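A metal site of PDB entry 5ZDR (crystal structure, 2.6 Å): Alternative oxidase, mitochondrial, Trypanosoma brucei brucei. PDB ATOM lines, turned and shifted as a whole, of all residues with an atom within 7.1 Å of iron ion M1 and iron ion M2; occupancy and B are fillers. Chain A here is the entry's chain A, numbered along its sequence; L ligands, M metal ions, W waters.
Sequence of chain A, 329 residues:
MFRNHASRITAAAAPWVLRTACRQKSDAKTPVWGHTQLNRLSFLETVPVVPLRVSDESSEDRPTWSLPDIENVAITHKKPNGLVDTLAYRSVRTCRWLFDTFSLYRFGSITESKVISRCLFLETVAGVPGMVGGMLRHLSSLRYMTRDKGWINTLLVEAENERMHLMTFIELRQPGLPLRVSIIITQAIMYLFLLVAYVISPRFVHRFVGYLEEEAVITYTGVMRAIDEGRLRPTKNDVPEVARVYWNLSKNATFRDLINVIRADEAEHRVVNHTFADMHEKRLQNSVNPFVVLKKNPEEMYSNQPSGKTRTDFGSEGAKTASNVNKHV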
ATOM      1  N   CYS A 119      13.427  -1.128  25.772  1.00  0.00           N
ATOM      2  CA  CYS A 119      13.840   0.267  25.567  1.00  0.00           C
ATOM      3  C   CYS A 119      12.862   1.260  26.249  1.00  0.00           C
ATOM      4  O   CYS A 119      13.275   2.157  26.987  1.00  0.00           O
ATOM      5  CB  CYS A 119      13.960   0.558  24.079  1.00  0.00           C
ATOM      6  SG  CYS A 119      14.785  -0.746  23.105  1.00  0.00           S
ATOM      7  N   LEU A 122      13.454   1.079  30.287  1.00  0.00           N
ATOM      8  CA  LEU A 122      14.756   1.601  30.605  1.00  0.00           C
ATOM      9  C   LEU A 122      14.871   3.059  30.254  1.00  0.00           C
ATOM     10  O   LEU A 122      15.474   3.820  31.004  1.00  0.00           O
ATOM     11  CB  LEU A 122      15.824   0.797  29.868  1.00  0.00           C
ATOM     12  CG  LEU A 122      16.109  -0.593  30.451  1.00  0.00           C
ATOM     13  CD1 LEU A 122      17.120  -1.273  29.586  1.00  0.00           C
ATOM     14  CD2 LEU A 122      16.640  -0.546  31.878  1.00  0.00           C
ATOM     15  N   GLU A 123      14.317   3.487  29.126  1.00  0.00           N
ATOM     16  CA  GLU A 123      14.384   4.913  28.797  1.00  0.00           C
ATOM     17  C   GLU A 123      13.712   5.768  29.876  1.00  0.00           C
ATOM     18  O   GLU A 123      14.143   6.888  30.092  1.00  0.00           O
ATOM     19  CB  GLU A 123      13.867   5.216  27.388  1.00  0.00           C
ATOM     20  CG  GLU A 123      14.810   4.740  26.255  1.00  0.00           C
ATOM     21  CD  GLU A 123      16.191   5.435  26.189  1.00  0.00           C
ATOM     22  OE1 GLU A 123      16.884   5.261  25.166  1.00  0.00           O
ATOM     23  OE2 GLU A 123      16.621   6.141  27.137  1.00  0.00           O
ATOM     24  N   ALA A 126      16.759   6.585  32.164  1.00  0.00           N
ATOM     25  CA  ALA A 126      17.862   7.312  31.520  1.00  0.00           C
ATOM     26  C   ALA A 126      17.626   8.838  31.525  1.00  0.00           C
ATOM     27  O   ALA A 126      18.571   9.645  31.448  1.00  0.00           O
ATOM     28  CB  ALA A 126      18.035   6.812  30.092  1.00  0.00           C
ATOM     29  N   GLY A 127      16.353   9.213  31.602  1.00  0.00           N
ATOM     30  CA  GLY A 127      16.003  10.609  31.733  1.00  0.00           C
ATOM     31  C   GLY A 127      16.316  11.270  33.057  1.00  0.00           C
ATOM     32  O   GLY A 127      16.239  12.500  33.136  1.00  0.00           O
ATOM     33  N   GLU A 158      20.496  16.345  27.498  1.00  0.00           N
ATOM     34  CA  GLU A 158      20.620  14.875  27.588  1.00  0.00           C
ATOM     35  C   GLU A 158      19.332  14.370  28.180  1.00  0.00           C
ATOM     36  O   GLU A 158      18.598  13.653  27.516  1.00  0.00           O
ATOM     37  CB  GLU A 158      21.808  14.423  28.486  1.00  0.00           C
ATOM     38  CG  GLU A 158      22.165  12.924  28.375  1.00  0.00           C
ATOM     39  CD  GLU A 158      22.597  12.249  29.699  1.00  0.00           C
ATOM     40  OE1 GLU A 158      23.717  11.685  29.760  1.00  0.00           O
ATOM     41  OE2 GLU A 158      21.819  12.252  30.686  1.00  0.00           O
ATOM     42  N   ASN A 161      16.787  14.748  25.623  1.00  0.00           N
ATOM     43  CA  ASN A 161      17.070  13.848  24.533  1.00  0.00           C
ATOM     44  C   ASN A 161      16.744  12.392  24.874  1.00  0.00           C
ATOM     45  O   ASN A 161      16.341  11.619  23.995  1.00  0.00           O
ATOM     46  CB  ASN A 161      18.551  14.043  24.173  1.00  0.00           C
ATOM     47  CG  ASN A 161      19.042  13.066  23.123  1.00  0.00           C
ATOM     48  OD1 ASN A 161      19.893  12.227  23.408  1.00  0.00           O
ATOM     49  ND2 ASN A 161      18.501  13.163  21.917  1.00  0.00           N
ATOM     50  N   GLU A 162      16.892  12.031  26.140  1.00  0.00           N
ATOM     51  CA  GLU A 162      16.451  10.713  26.636  1.00  0.00           C
ATOM     52  C   GLU A 162      14.932  10.678  26.897  1.00  0.00           C
ATOM     53  O   GLU A 162      14.256   9.646  26.732  1.00  0.00           O
ATOM     54  CB  GLU A 162      17.221  10.328  27.883  1.00  0.00           C
ATOM     55  CG  GLU A 162      18.728  10.193  27.714  1.00  0.00           C
ATOM     56  CD  GLU A 162      19.140   8.877  27.100  1.00  0.00           C
ATOM     57  OE1 GLU A 162      18.679   8.581  25.971  1.00  0.00           O
ATOM     58  OE2 GLU A 162      19.939   8.150  27.736  1.00  0.00           O
ATOM     59  N   ARG A 163      14.378  11.814  27.288  1.00  0.00           N
ATOM     60  CA  ARG A 163      12.942  11.869  27.434  1.00  0.00           C
ATOM     61  C   ARG A 163      12.343  11.678  26.051  1.00  0.00           C
ATOM     62  O   ARG A 163      11.347  10.946  25.920  1.00  0.00           O
ATOM     63  CB  ARG A 163      12.470  13.172  28.102  1.00  0.00           C
ATOM     64  CG  ARG A 163      10.996  13.129  28.460  1.00  0.00           C
ATOM     65  CD  ARG A 163      10.474  14.400  29.110  1.00  0.00           C
ATOM     66  NE  ARG A 163      10.596  15.597  28.259  1.00  0.00           N
ATOM     67  CZ  ARG A 163       9.776  15.924  27.264  1.00  0.00           C
ATOM     68  NH1 ARG A 163      10.013  17.024  26.568  1.00  0.00           N
ATOM     69  NH2 ARG A 163       8.735  15.141  26.935  1.00  0.00           N
ATOM     70  N   HIS A 165      13.536   9.828  23.801  1.00  0.00           N
ATOM     71  CA  HIS A 165      13.652   8.398  23.541  1.00  0.00           C
ATOM     72  C   HIS A 165      12.456   7.625  24.090  1.00  0.00           C
ATOM     73  O   HIS A 165      11.907   6.718  23.429  1.00  0.00           O
ATOM     74  CB  HIS A 165      14.945   7.909  24.164  1.00  0.00           C
ATOM     75  CG  HIS A 165      16.172   8.351  23.405  1.00  0.00           C
ATOM     76  ND1 HIS A 165      17.431   7.870  23.689  1.00  0.00           N
ATOM     77  CD2 HIS A 165      16.310   9.167  22.334  1.00  0.00           C
ATOM     78  CE1 HIS A 165      18.295   8.396  22.846  1.00  0.00           C
ATOM     79  NE2 HIS A 165      17.634   9.172  22.013  1.00  0.00           N
ATOM     80  N   LEU A 166      12.010   7.995  25.291  1.00  0.00           N
ATOM     81  CA  LEU A 166      10.746   7.522  25.812  1.00  0.00           C
ATOM     82  C   LEU A 166       9.627   7.872  24.851  1.00  0.00           C
ATOM     83  O   LEU A 166       8.829   7.016  24.511  1.00  0.00           O
ATOM     84  CB  LEU A 166      10.420   8.149  27.166  1.00  0.00           C
ATOM     85  CG  LEU A 166       9.826   7.197  28.208  1.00  0.00           C
ATOM     86  CD1 LEU A 166       9.003   7.978  29.194  1.00  0.00           C
ATOM     87  CD2 LEU A 166       8.990   6.085  27.570  1.00  0.00           C
ATOM     88  N   PHE A 169       9.336   5.617  21.670  1.00  0.00           N
ATOM     89  CA  PHE A 169       8.926   4.245  21.955  1.00  0.00           C
ATOM     90  C   PHE A 169       7.477   4.127  22.453  1.00  0.00           C
ATOM     91  O   PHE A 169       6.800   3.125  22.178  1.00  0.00           O
ATOM     92  CB  PHE A 169       9.892   3.579  22.934  1.00  0.00           C
ATOM     93  CG  PHE A 169      11.308   3.469  22.438  1.00  0.00           C
ATOM     94  CD1 PHE A 169      11.562   3.056  21.147  1.00  0.00           C
ATOM     95  CD2 PHE A 169      12.368   3.766  23.269  1.00  0.00           C
ATOM     96  CE1 PHE A 169      12.876   2.940  20.686  1.00  0.00           C
ATOM     97  CE2 PHE A 169      13.678   3.664  22.828  1.00  0.00           C
ATOM     98  CZ  PHE A 169      13.932   3.251  21.527  1.00  0.00           C
ATOM     99  N   VAL A 209      26.659   6.651  34.619  1.00  0.00           N
ATOM    100  CA  VAL A 209      26.061   6.872  33.265  1.00  0.00           C
ATOM    101  C   VAL A 209      27.082   6.558  32.127  1.00  0.00           C
ATOM    102  O   VAL A 209      26.737   6.040  31.034  1.00  0.00           O
ATOM    103  CB  VAL A 209      25.607   8.333  33.100  1.00  0.00           C
ATOM    104  CG1 VAL A 209      24.938   8.522  31.768  1.00  0.00           C
ATOM    105  CG2 VAL A 209      24.655   8.724  34.213  1.00  0.00           C
ATOM    106  N   LEU A 212      26.494   2.777  32.220  1.00  0.00           N
ATOM    107  CA  LEU A 212      25.131   2.670  31.753  1.00  0.00           C
ATOM    108  C   LEU A 212      25.067   2.749  30.214  1.00  0.00           C
ATOM    109  O   LEU A 212      24.626   1.811  29.547  1.00  0.00           O
ATOM    110  CB  LEU A 212      24.326   3.821  32.356  1.00  0.00           C
ATOM    111  CG  LEU A 212      23.207   3.646  33.380  1.00  0.00           C
ATOM    112  CD1 LEU A 212      22.121   4.571  32.885  1.00  0.00           C
ATOM    113  CD2 LEU A 212      22.667   2.231  33.460  1.00  0.00           C
ATOM    114  N   GLU A 213      25.538   3.861  29.637  1.00  0.00           N
ATOM    115  CA  GLU A 213      25.544   4.008  28.154  1.00  0.00           C
ATOM    116  C   GLU A 213      26.433   3.001  27.377  1.00  0.00           C
ATOM    117  O   GLU A 213      26.163   2.690  26.209  1.00  0.00           O
ATOM    118  CB  GLU A 213      25.966   5.439  27.769  1.00  0.00           C
ATOM    119  CG  GLU A 213      25.141   6.567  28.403  1.00  0.00           C
ATOM    120  CD  GLU A 213      23.741   6.621  27.877  1.00  0.00           C
ATOM    121  OE1 GLU A 213      23.187   5.540  27.717  1.00  0.00           O
ATOM    122  OE2 GLU A 213      23.206   7.718  27.607  1.00  0.00           O
ATOM    123  N   ALA A 216      23.973   0.546  26.910  1.00  0.00           N
ATOM    124  CA  ALA A 216      22.969   1.041  25.953  1.00  0.00           C
ATOM    125  C   ALA A 216      23.468   0.895  24.519  1.00  0.00           C
ATOM    126  O   ALA A 216      22.660   0.596  23.616  1.00  0.00           O
ATOM    127  CB  ALA A 216      22.692   2.506  26.230  1.00  0.00           C
ATOM    128  N   TYR A 220      21.844  -1.765  21.551  1.00  0.00           N
ATOM    129  CA  TYR A 220      21.283  -1.270  20.294  1.00  0.00           C
ATOM    130  C   TYR A 220      22.024  -1.762  19.050  1.00  0.00           C
ATOM    131  O   TYR A 220      21.361  -2.024  18.031  1.00  0.00           O
ATOM    132  CB  TYR A 220      21.170   0.263  20.273  1.00  0.00           C
ATOM    133  CG  TYR A 220      20.004   0.882  21.055  1.00  0.00           C
ATOM    134  CD1 TYR A 220      18.690   0.513  20.827  1.00  0.00           C
ATOM    135  CD2 TYR A 220      20.246   1.890  21.991  1.00  0.00           C
ATOM    136  CE1 TYR A 220      17.655   1.111  21.523  1.00  0.00           C
ATOM    137  CE2 TYR A 220      19.224   2.471  22.697  1.00  0.00           C
ATOM    138  CZ  TYR A 220      17.928   2.093  22.458  1.00  0.00           C
ATOM    139  OH  TYR A 220      16.911   2.727  23.173  1.00  0.00           O
ATOM    140  N   ILE A 262      19.168   6.791  17.727  1.00  0.00           N
ATOM    141  CA  ILE A 262      19.096   6.554  19.193  1.00  0.00           C
ATOM    142  C   ILE A 262      20.415   5.941  19.775  1.00  0.00           C
ATOM    143  O   ILE A 262      20.820   6.263  20.866  1.00  0.00           O
ATOM    144  CB  ILE A 262      17.869   5.691  19.553  1.00  0.00           C
ATOM    145  CG1 ILE A 262      16.600   6.562  19.538  1.00  0.00           C
ATOM    146  CG2 ILE A 262      18.008   5.049  20.941  1.00  0.00           C
ATOM    147  CD1 ILE A 262      15.311   5.778  19.641  1.00  0.00           C
ATOM    148  N   ASP A 265      23.252   8.988  19.721  1.00  0.00           N
ATOM    149  CA  ASP A 265      22.966   9.705  20.993  1.00  0.00           C
ATOM    150  C   ASP A 265      23.601   9.064  22.268  1.00  0.00           C
ATOM    151  O   ASP A 265      24.044   9.775  23.205  1.00  0.00           O
ATOM    152  CB  ASP A 265      21.456   9.809  21.173  1.00  0.00           C
ATOM    153  CG  ASP A 265      20.806  10.912  20.277  1.00  0.00           C
ATOM    154  OD1 ASP A 265      21.573  11.701  19.638  1.00  0.00           O
ATOM    155  OD2 ASP A 265      19.537  11.004  20.255  1.00  0.00           O
ATOM    156  N   GLU A 266      23.682   7.737  22.329  1.00  0.00           N
ATOM    157  CA  GLU A 266      24.097   7.102  23.594  1.00  0.00           C
ATOM    158  C   GLU A 266      25.605   7.017  23.635  1.00  0.00           C
ATOM    159  O   GLU A 266      26.235   7.050  24.697  1.00  0.00           O
ATOM    160  CB  GLU A 266      23.437   5.749  23.800  1.00  0.00           C
ATOM    161  CG  GLU A 266      21.929   5.694  23.510  1.00  0.00           C
ATOM    162  CD  GLU A 266      21.000   6.153  24.632  1.00  0.00           C
ATOM    163  OE1 GLU A 266      19.763   6.222  24.339  1.00  0.00           O
ATOM    164  OE2 GLU A 266      21.422   6.412  25.793  1.00  0.00           O
ATOM    165  N   HIS A 269      26.625  10.451  25.065  1.00  0.00           N
ATOM    166  CA  HIS A 269      26.404  10.529  26.497  1.00  0.00           C
ATOM    167  C   HIS A 269      27.450   9.730  27.232  1.00  0.00           C
ATOM    168  O   HIS A 269      27.985  10.165  28.257  1.00  0.00           O
ATOM    169  CB  HIS A 269      25.046   9.951  26.812  1.00  0.00           C
ATOM    170  CG  HIS A 269      23.910  10.651  26.141  1.00  0.00           C
ATOM    171  ND1 HIS A 269      22.661  10.086  26.001  1.00  0.00           N
ATOM    172  CD2 HIS A 269      23.825  11.878  25.570  1.00  0.00           C
ATOM    173  CE1 HIS A 269      21.857  10.937  25.384  1.00  0.00           C
ATOM    174  NE2 HIS A 269      22.544  12.031  25.118  1.00  0.00           N
ATOM    175  N   ARG A 270      27.708   8.524  26.705  1.00  0.00           N
ATOM    176  CA  ARG A 270      28.861   7.698  27.135  1.00  0.00           C
ATOM    177  C   ARG A 270      30.148   8.523  27.283  1.00  0.00           C
ATOM    178  O   ARG A 270      30.776   8.480  28.355  1.00  0.00           O
ATOM    179  CB  ARG A 270      29.075   6.534  26.139  1.00  0.00           C
ATOM    180  CG  ARG A 270      30.241   5.609  26.439  1.00  0.00           C
ATOM    181  CD  ARG A 270      30.341   4.466  25.408  1.00  0.00           C
ATOM    182  NE  ARG A 270      30.604   4.948  24.042  1.00  0.00           N
ATOM    183  CZ  ARG A 270      30.525   4.201  22.938  1.00  0.00           C
ATOM    184  NH1 ARG A 270      30.194   2.918  23.018  1.00  0.00           N
ATOM    185  NH2 ARG A 270      30.809   4.732  21.751  1.00  0.00           N
HETATM  186  O1  LIG L   1      19.165   5.762  26.671  1.00  0.00           O
HETATM  187  O1  LG2 L   2      21.408   0.851  30.481  1.00  0.00           O
HETATM  188  C1  LG2 L   2      20.662   0.539  29.375  1.00  0.00           C
HETATM  189  C2  LG2 L   2      20.683  -0.742  28.839  1.00  0.00           C
HETATM  190  C3  LG2 L   2      21.495  -1.808  29.486  1.00  0.00           C
HETATM  191  C4  LG2 L   2      20.729  -2.193  30.725  1.00  0.00           C
HETATM  192  C5  LG2 L   2      21.276  -2.093  31.930  1.00  0.00           C
HETATM  193  C6  LG2 L   2      20.467  -2.469  33.130  1.00  0.00           C
HETATM  194  C7  LG2 L   2      19.987  -1.207  33.798  1.00  0.00           C
HETATM  195  C8  LG2 L   2      18.970  -1.609  34.848  1.00  0.00           C
HETATM  196  C9  LG2 L   2      18.422  -0.731  35.701  1.00  0.00           C
HETATM  197  C10 LG2 L   2      17.422  -1.231  36.710  1.00  0.00           C
HETATM  198  O2  LG2 L   2      17.007  -0.120  37.495  1.00  0.00           O
HETATM  199  O3  LG2 L   2      20.826   2.986  30.339  1.00  0.00           O
HETATM  200  C11 LG2 L   2      19.989   2.879  29.447  1.00  0.00           C
HETATM  201  C12 LG2 L   2      19.899   1.539  28.816  1.00  0.00           C
HETATM  202  C13 LG2 L   2      19.929  -1.050  27.754  1.00  0.00           C
HETATM  203  O4  LG2 L   2      19.952  -2.308  27.267  1.00  0.00           O
HETATM  204  C14 LG2 L   2      22.692  -1.628  32.163  1.00  0.00           C
HETATM  205  C15 LG2 L   2      18.780   0.740  35.688  1.00  0.00           C
HETATM  206  C16 LG2 L   2      16.207  -1.861  36.028  1.00  0.00           C
HETATM  207  C17 LG2 L   2      19.087   1.212  27.633  1.00  0.00           C
HETATM  208  C18 LG2 L   2      19.126  -0.086  27.176  1.00  0.00           C
HETATM  209 CL1  LG2 L   2      18.143  -0.559  25.762  1.00  0.00          CL
HETATM  210  C19 LG2 L   2      18.215   2.206  26.929  1.00  0.00           C
HETATM  211 FE    FE M   1      21.102   6.501  27.899  1.00  0.00          FE
HETATM  212 FE    FE M   2      18.270   6.732  25.477  1.00  0.00          FE
HETATM  213  O   HOH W   1      21.470   6.245  30.466  1.00  0.00           O
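Iron ion M1 is bound by the side-chain carboxylate (OE2) of Glu 162, the side-chain carboxylate (OE2) of Glu 266, the side-chain carboxylate (OE1) of Glu 213, an oxygen (O1) of LIG L1 and the side-chain carboxylate (OE2) of Glu 213. Iron ion M1 has five donor atoms within binding distance. Slightly farther from iron ion M1 lies water W1 (2.6 Å).
The backbone carbonyl oxygen (O) of Leu 212 sits at hydrogen-bond distance from an oxygen (O1) of LG2 L2.
Residues that only touch iron ion M1: Ala 126. Four residues have an atom within 4 Å of iron ion M1: Ala 126, Glu 162, Glu 213 and Glu 266.
The side-chain hydroxyl (OH) of Tyr 220 lies close to the side-chain carboxylate (OE1) of Glu 123. The backbone carbonyl oxygen of Asn 161 lies close to a ring nitrogen (NE2) of His 165, at 3.4 Å. A ring nitrogen (NE2) of His 165 lies within hydrogen-bond range of the side-chain carboxylate (OD2) of Asp 265 (3.2 Å). The side-chain carboxylate (OE2) of Glu 213 sits close to a ring nitrogen (ND1) of His 269 (2.9 Å).
Iron ion M2 is bound by O1 of LIG L1 (1.8 Å), OE1 of Glu 266 (1.9 Å), OE1 of Glu 162 (2.0 Å), OE1 of Glu 123 (2.0 Å), ND1 of His 165 (2.3 Å) and OE2 of Glu 123 (2.4 Å).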
